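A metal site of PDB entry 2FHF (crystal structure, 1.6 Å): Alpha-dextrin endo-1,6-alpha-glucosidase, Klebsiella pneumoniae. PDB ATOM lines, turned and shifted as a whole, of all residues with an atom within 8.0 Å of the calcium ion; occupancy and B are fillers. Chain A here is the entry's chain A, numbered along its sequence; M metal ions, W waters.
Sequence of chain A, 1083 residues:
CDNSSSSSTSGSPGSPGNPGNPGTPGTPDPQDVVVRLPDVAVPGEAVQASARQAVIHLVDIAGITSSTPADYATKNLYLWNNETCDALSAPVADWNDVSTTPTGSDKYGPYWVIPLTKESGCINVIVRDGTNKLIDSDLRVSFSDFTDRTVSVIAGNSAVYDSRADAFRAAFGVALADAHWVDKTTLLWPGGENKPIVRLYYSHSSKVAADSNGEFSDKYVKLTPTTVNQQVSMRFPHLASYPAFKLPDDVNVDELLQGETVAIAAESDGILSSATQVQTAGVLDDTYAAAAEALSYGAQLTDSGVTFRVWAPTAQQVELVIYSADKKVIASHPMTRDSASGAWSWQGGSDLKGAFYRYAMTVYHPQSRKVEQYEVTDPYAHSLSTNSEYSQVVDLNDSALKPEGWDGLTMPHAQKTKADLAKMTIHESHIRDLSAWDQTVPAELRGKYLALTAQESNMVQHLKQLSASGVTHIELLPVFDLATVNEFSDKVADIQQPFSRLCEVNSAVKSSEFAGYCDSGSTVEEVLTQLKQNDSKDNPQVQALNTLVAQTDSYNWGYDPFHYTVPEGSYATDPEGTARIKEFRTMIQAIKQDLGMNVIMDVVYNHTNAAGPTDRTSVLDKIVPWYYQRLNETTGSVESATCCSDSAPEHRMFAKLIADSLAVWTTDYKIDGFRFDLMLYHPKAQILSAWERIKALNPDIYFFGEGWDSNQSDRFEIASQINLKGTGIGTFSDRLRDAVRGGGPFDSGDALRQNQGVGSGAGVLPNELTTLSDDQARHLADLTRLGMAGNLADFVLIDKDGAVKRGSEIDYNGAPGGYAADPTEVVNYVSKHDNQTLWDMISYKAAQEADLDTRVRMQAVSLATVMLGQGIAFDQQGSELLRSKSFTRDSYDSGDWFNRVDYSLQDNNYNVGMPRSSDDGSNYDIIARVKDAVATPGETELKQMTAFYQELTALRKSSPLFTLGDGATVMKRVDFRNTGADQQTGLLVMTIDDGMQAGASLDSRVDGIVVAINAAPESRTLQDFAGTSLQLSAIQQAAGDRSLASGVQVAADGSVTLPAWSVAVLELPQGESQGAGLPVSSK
Within 4 Å of the calcium ion: Asp 148, Thr 150 and Asp 162.
The nearest printed residue that does not touch the calcium ion is Ser 163 (4.6 Å).
The side-chain hydroxyl (OG1) of Thr 150 is in hydrogen-bond range of the backbone NH (N) of Ala 49, at 2.9 Å.
The calcium ion is bound by the backbone carbonyl oxygen (O) of Asp 162, at 2.3 Å.
The calcium ion is bound by water W1, at 2.3 Å.
The calcium ion is bound by OD2 of Asp 162 (2.4 Å).
The calcium ion is bound by OD1 of Asp 148.
The backbone carbonyl oxygen (O) of Thr 150 binds the calcium ion (2.5 Å).
The side-chain carboxylate (OD2) of Asp 148 is bound to the calcium ion.
Water W1 lies within hydrogen-bond range of the side-chain carboxylate of Glu 45 (2.9 Å) and the side-chain amide nitrogen of Gln 48 (2.9 Å).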
ATOM      1  N   GLU A  45      15.140   2.512 -26.610  1.00  0.00           N
ATOM      2  CA  GLU A  45      15.046   2.808 -25.185  1.00  0.00           C
ATOM      3  C   GLU A  45      15.706   1.703 -24.371  1.00  0.00           C
ATOM      4  O   GLU A  45      15.533   0.520 -24.655  1.00  0.00           O
ATOM      5  CB  GLU A  45      13.573   2.949 -24.771  1.00  0.00           C
ATOM      6  CG  GLU A  45      12.859   4.098 -25.468  1.00  0.00           C
ATOM      7  CD  GLU A  45      13.469   5.437 -25.137  1.00  0.00           C
ATOM      8  OE1 GLU A  45      13.209   5.966 -24.029  1.00  0.00           O
ATOM      9  OE2 GLU A  45      14.225   5.977 -25.978  1.00  0.00           O
ATOM     10  N   VAL A  47      15.144   1.123 -21.198  1.00  0.00           N
ATOM     11  CA  VAL A  47      14.107   0.559 -20.338  1.00  0.00           C
ATOM     12  C   VAL A  47      12.974   1.566 -20.157  1.00  0.00           C
ATOM     13  O   VAL A  47      13.187   2.770 -20.271  1.00  0.00           O
ATOM     14  CB  VAL A  47      14.682   0.199 -18.949  1.00  0.00           C
ATOM     15  CG1 VAL A  47      15.253   1.447 -18.282  1.00  0.00           C
ATOM     16  CG2 VAL A  47      13.608  -0.429 -18.074  1.00  0.00           C
ATOM     17  N   GLN A  48      11.776   1.060 -19.880  1.00  0.00           N
ATOM     18  CA  GLN A  48      10.613   1.923 -19.675  1.00  0.00           C
ATOM     19  C   GLN A  48      10.289   2.007 -18.182  1.00  0.00           C
ATOM     20  O   GLN A  48      10.471   1.045 -17.441  1.00  0.00           O
ATOM     21  CB  GLN A  48       9.399   1.355 -20.423  1.00  0.00           C
ATOM     22  CG  GLN A  48       9.513   1.414 -21.938  1.00  0.00           C
ATOM     23  CD  GLN A  48       9.470   2.825 -22.477  1.00  0.00           C
ATOM     24  OE1 GLN A  48       8.506   3.564 -22.250  1.00  0.00           O
ATOM     25  NE2 GLN A  48      10.519   3.227 -23.190  1.00  0.00           N
ATOM     26  N   ALA A  49       9.828   3.175 -17.746  1.00  0.00           N
ATOM     27  CA  ALA A  49       9.481   3.380 -16.342  1.00  0.00           C
ATOM     28  C   ALA A  49       8.264   2.530 -15.985  1.00  0.00           C
ATOM     29  O   ALA A  49       7.277   2.502 -16.722  1.00  0.00           O
ATOM     30  CB  ALA A  49       9.180   4.846 -16.087  1.00  0.00           C
ATOM     31  N   VAL A  55      12.254   7.171 -15.213  1.00  0.00           N
ATOM     32  CA  VAL A  55      13.495   6.724 -15.822  1.00  0.00           C
ATOM     33  C   VAL A  55      14.121   7.855 -16.639  1.00  0.00           C
ATOM     34  O   VAL A  55      13.433   8.516 -17.416  1.00  0.00           O
ATOM     35  CB  VAL A  55      13.263   5.508 -16.744  1.00  0.00           C
ATOM     36  CG1 VAL A  55      14.557   5.158 -17.487  1.00  0.00           C
ATOM     37  CG2 VAL A  55      12.804   4.310 -15.926  1.00  0.00           C
ATOM     38  N   HIS A  57      17.358   8.766 -19.239  1.00  0.00           N
ATOM     39  CA  HIS A  57      18.431   8.280 -20.103  1.00  0.00           C
ATOM     40  C   HIS A  57      19.427   9.401 -20.370  1.00  0.00           C
ATOM     41  O   HIS A  57      19.046  10.557 -20.560  1.00  0.00           O
ATOM     42  CB  HIS A  57      17.859   7.837 -21.462  1.00  0.00           C
ATOM     43  CG  HIS A  57      16.899   6.682 -21.374  1.00  0.00           C
ATOM     44  ND1 HIS A  57      17.319   5.387 -21.145  1.00  0.00           N
ATOM     45  CD2 HIS A  57      15.556   6.633 -21.517  1.00  0.00           C
ATOM     46  CE1 HIS A  57      16.267   4.588 -21.144  1.00  0.00           C
ATOM     47  NE2 HIS A  57      15.188   5.315 -21.368  1.00  0.00           N
ATOM     48  N   ASP A 145       3.848  16.119 -19.362  1.00  0.00           N
ATOM     49  CA  ASP A 145       4.494  16.338 -20.652  1.00  0.00           C
ATOM     50  C   ASP A 145       4.987  14.994 -21.180  1.00  0.00           C
ATOM     51  O   ASP A 145       4.931  14.732 -22.385  1.00  0.00           O
ATOM     52  CB  ASP A 145       5.672  17.296 -20.498  1.00  0.00           C
ATOM     53  CG  ASP A 145       5.240  18.709 -20.173  1.00  0.00           C
ATOM     54  OD1 ASP A 145       4.523  18.901 -19.169  1.00  0.00           O
ATOM     55  OD2 ASP A 145       5.635  19.639 -20.912  1.00  0.00           O
ATOM     56  N   PHE A 146       5.459  14.142 -20.274  1.00  0.00           N
ATOM     57  CA  PHE A 146       5.957  12.816 -20.631  1.00  0.00           C
ATOM     58  C   PHE A 146       5.231  11.776 -19.790  1.00  0.00           C
ATOM     59  O   PHE A 146       5.693  11.382 -18.721  1.00  0.00           O
ATOM     60  CB  PHE A 146       7.465  12.736 -20.398  1.00  0.00           C
ATOM     61  CG  PHE A 146       8.244  13.827 -21.074  1.00  0.00           C
ATOM     62  CD1 PHE A 146       8.338  15.088 -20.503  1.00  0.00           C
ATOM     63  CD2 PHE A 146       8.870  13.601 -22.296  1.00  0.00           C
ATOM     64  CE1 PHE A 146       9.039  16.112 -21.136  1.00  0.00           C
ATOM     65  CE2 PHE A 146       9.582  14.616 -22.939  1.00  0.00           C
ATOM     66  CZ  PHE A 146       9.656  15.876 -22.359  1.00  0.00           C
ATOM     67  N   THR A 147       4.079  11.329 -20.290  1.00  0.00           N
ATOM     68  CA  THR A 147       3.249  10.353 -19.595  1.00  0.00           C
ATOM     69  C   THR A 147       3.974   9.109 -19.080  1.00  0.00           C
ATOM     70  O   THR A 147       3.831   8.753 -17.907  1.00  0.00           O
ATOM     71  CB  THR A 147       2.078   9.902 -20.498  1.00  0.00           C
ATOM     72  OG1 THR A 147       1.300   8.911 -19.810  1.00  0.00           O
ATOM     73  CG2 THR A 147       2.600   9.309 -21.808  1.00  0.00           C
ATOM     74  N   ASP A 148       4.758   8.458 -19.941  1.00  0.00           N
ATOM     75  CA  ASP A 148       5.470   7.244 -19.537  1.00  0.00           C
ATOM     76  C   ASP A 148       6.611   7.490 -18.551  1.00  0.00           C
ATOM     77  O   ASP A 148       7.333   6.560 -18.189  1.00  0.00           O
ATOM     78  CB  ASP A 148       6.018   6.511 -20.768  1.00  0.00           C
ATOM     79  CG  ASP A 148       6.929   7.385 -21.620  1.00  0.00           C
ATOM     80  OD1 ASP A 148       7.817   8.040 -21.054  1.00  0.00           O
ATOM     81  OD2 ASP A 148       6.741   7.404 -22.847  1.00  0.00           O
ATOM     82  N   ARG A 149       6.767   8.729 -18.106  1.00  0.00           N
ATOM     83  CA  ARG A 149       7.810   9.098 -17.155  1.00  0.00           C
ATOM     84  C   ARG A 149       9.182   8.526 -17.497  1.00  0.00           C
ATOM     85  O   ARG A 149       9.965   8.193 -16.614  1.00  0.00           O
ATOM     86  CB  ARG A 149       7.405   8.646 -15.743  1.00  0.00           C
ATOM     87  CG  ARG A 149       6.091   9.240 -15.255  1.00  0.00           C
ATOM     88  CD  ARG A 149       5.868   8.962 -13.774  1.00  0.00           C
ATOM     89  NE  ARG A 149       5.870   7.531 -13.470  1.00  0.00           N
ATOM     90  CZ  ARG A 149       4.957   6.671 -13.902  1.00  0.00           C
ATOM     91  NH1 ARG A 149       3.956   7.085 -14.659  1.00  0.00           N
ATOM     92  NH2 ARG A 149       5.046   5.388 -13.567  1.00  0.00           N
ATOM     93  N   THR A 150       9.471   8.435 -18.792  1.00  0.00           N
ATOM     94  CA  THR A 150      10.757   7.918 -19.259  1.00  0.00           C
ATOM     95  C   THR A 150      11.352   8.950 -20.221  1.00  0.00           C
ATOM     96  O   THR A 150      10.953   9.019 -21.383  1.00  0.00           O
ATOM     97  CB  THR A 150      10.582   6.583 -20.009  1.00  0.00           C
ATOM     98  OG1 THR A 150       9.878   5.656 -19.173  1.00  0.00           O
ATOM     99  CG2 THR A 150      11.937   5.990 -20.383  1.00  0.00           C
ATOM    100  N   VAL A 151      12.296   9.741 -19.728  1.00  0.00           N
ATOM    101  CA  VAL A 151      12.917  10.792 -20.537  1.00  0.00           C
ATOM    102  C   VAL A 151      14.380  10.568 -20.873  1.00  0.00           C
ATOM    103  O   VAL A 151      15.020   9.648 -20.367  1.00  0.00           O
ATOM    104  CB  VAL A 151      12.791  12.152 -19.829  1.00  0.00           C
ATOM    105  CG1 VAL A 151      11.317  12.477 -19.592  1.00  0.00           C
ATOM    106  CG2 VAL A 151      13.556  12.130 -18.508  1.00  0.00           C
ATOM    107  N   SER A 152      14.910  11.432 -21.734  1.00  0.00           N
ATOM    108  CA  SER A 152      16.298  11.364 -22.162  1.00  0.00           C
ATOM    109  C   SER A 152      16.881  12.761 -22.323  1.00  0.00           C
ATOM    110  O   SER A 152      16.193  13.695 -22.742  1.00  0.00           O
ATOM    111  CB  SER A 152      16.412  10.606 -23.487  1.00  0.00           C
ATOM    112  OG  SER A 152      15.917   9.289 -23.378  1.00  0.00           O
ATOM    113  N   TYR A 161      13.816  15.176 -23.356  1.00  0.00           N
ATOM    114  CA  TYR A 161      13.205  14.464 -24.464  1.00  0.00           C
ATOM    115  C   TYR A 161      12.443  13.238 -23.991  1.00  0.00           C
ATOM    116  O   TYR A 161      12.738  12.680 -22.930  1.00  0.00           O
ATOM    117  CB  TYR A 161      14.283  14.061 -25.476  1.00  0.00           C
ATOM    118  CG  TYR A 161      15.017  15.248 -26.062  1.00  0.00           C
ATOM    119  CD1 TYR A 161      14.396  16.087 -26.981  1.00  0.00           C
ATOM    120  CD2 TYR A 161      16.319  15.558 -25.655  1.00  0.00           C
ATOM    121  CE1 TYR A 161      15.050  17.205 -27.494  1.00  0.00           C
ATOM    122  CE2 TYR A 161      16.981  16.677 -26.158  1.00  0.00           C
ATOM    123  CZ  TYR A 161      16.342  17.495 -27.078  1.00  0.00           C
ATOM    124  OH  TYR A 161      16.984  18.611 -27.573  1.00  0.00           O
ATOM    125  N   ASP A 162      11.463  12.811 -24.789  1.00  0.00           N
ATOM    126  CA  ASP A 162      10.626  11.661 -24.460  1.00  0.00           C
ATOM    127  C   ASP A 162      11.284  10.327 -24.806  1.00  0.00           C
ATOM    128  O   ASP A 162      10.841   9.278 -24.344  1.00  0.00           O
ATOM    129  CB  ASP A 162       9.284  11.774 -25.181  1.00  0.00           C
ATOM    130  CG  ASP A 162       8.197  10.919 -24.543  1.00  0.00           C
ATOM    131  OD1 ASP A 162       7.091  10.839 -25.120  1.00  0.00           O
ATOM    132  OD2 ASP A 162       8.453  10.338 -23.475  1.00  0.00           O
ATOM    133  N   SER A 163      12.321  10.369 -25.629  1.00  0.00           N
ATOM    134  CA  SER A 163      13.025   9.150 -26.028  1.00  0.00           C
ATOM    135  C   SER A 163      14.462   9.438 -26.434  1.00  0.00           C
ATOM    136  O   SER A 163      14.801  10.557 -26.791  1.00  0.00           O
ATOM    137  CB  SER A 163      12.296   8.480 -27.204  1.00  0.00           C
ATOM    138  OG  SER A 163      12.362   9.271 -28.373  1.00  0.00           O
ATOM    139  N   ARG A 164      15.306   8.413 -26.376  1.00  0.00           N
ATOM    140  CA  ARG A 164      16.711   8.567 -26.747  1.00  0.00           C
ATOM    141  C   ARG A 164      16.814   8.845 -28.237  1.00  0.00           C
ATOM    142  O   ARG A 164      17.801   9.407 -28.700  1.00  0.00           O
ATOM    143  CB  ARG A 164      17.511   7.301 -26.388  1.00  0.00           C
ATOM    144  CG  ARG A 164      17.606   7.049 -24.892  1.00  0.00           C
ATOM    145  CD  ARG A 164      18.770   6.125 -24.527  1.00  0.00           C
ATOM    146  NE  ARG A 164      18.574   4.753 -24.978  1.00  0.00           N
ATOM    147  CZ  ARG A 164      19.376   3.739 -24.653  1.00  0.00           C
ATOM    148  NH1 ARG A 164      20.426   3.952 -23.875  1.00  0.00           N
ATOM    149  NH2 ARG A 164      19.129   2.513 -25.104  1.00  0.00           N
ATOM    150  N   ASP A 166      14.533  10.747 -30.006  1.00  0.00           N
ATOM    151  CA  ASP A 166      14.211  12.159 -30.185  1.00  0.00           C
ATOM    152  C   ASP A 166      15.432  13.006 -29.830  1.00  0.00           C
ATOM    153  O   ASP A 166      15.798  13.924 -30.571  1.00  0.00           O
ATOM    154  CB  ASP A 166      13.042  12.557 -29.290  1.00  0.00           C
ATOM    155  CG  ASP A 166      11.715  12.035 -29.795  1.00  0.00           C
ATOM    156  OD1 ASP A 166      10.689  12.248 -29.115  1.00  0.00           O
ATOM    157  OD2 ASP A 166      11.689  11.422 -30.887  1.00  0.00           O
HETATM  158 CA    CA M   1       9.286   8.131 -23.077  1.00  0.00          CA
HETATM  159  O   HOH W   1      10.408   6.145 -23.525  1.00  0.00           O
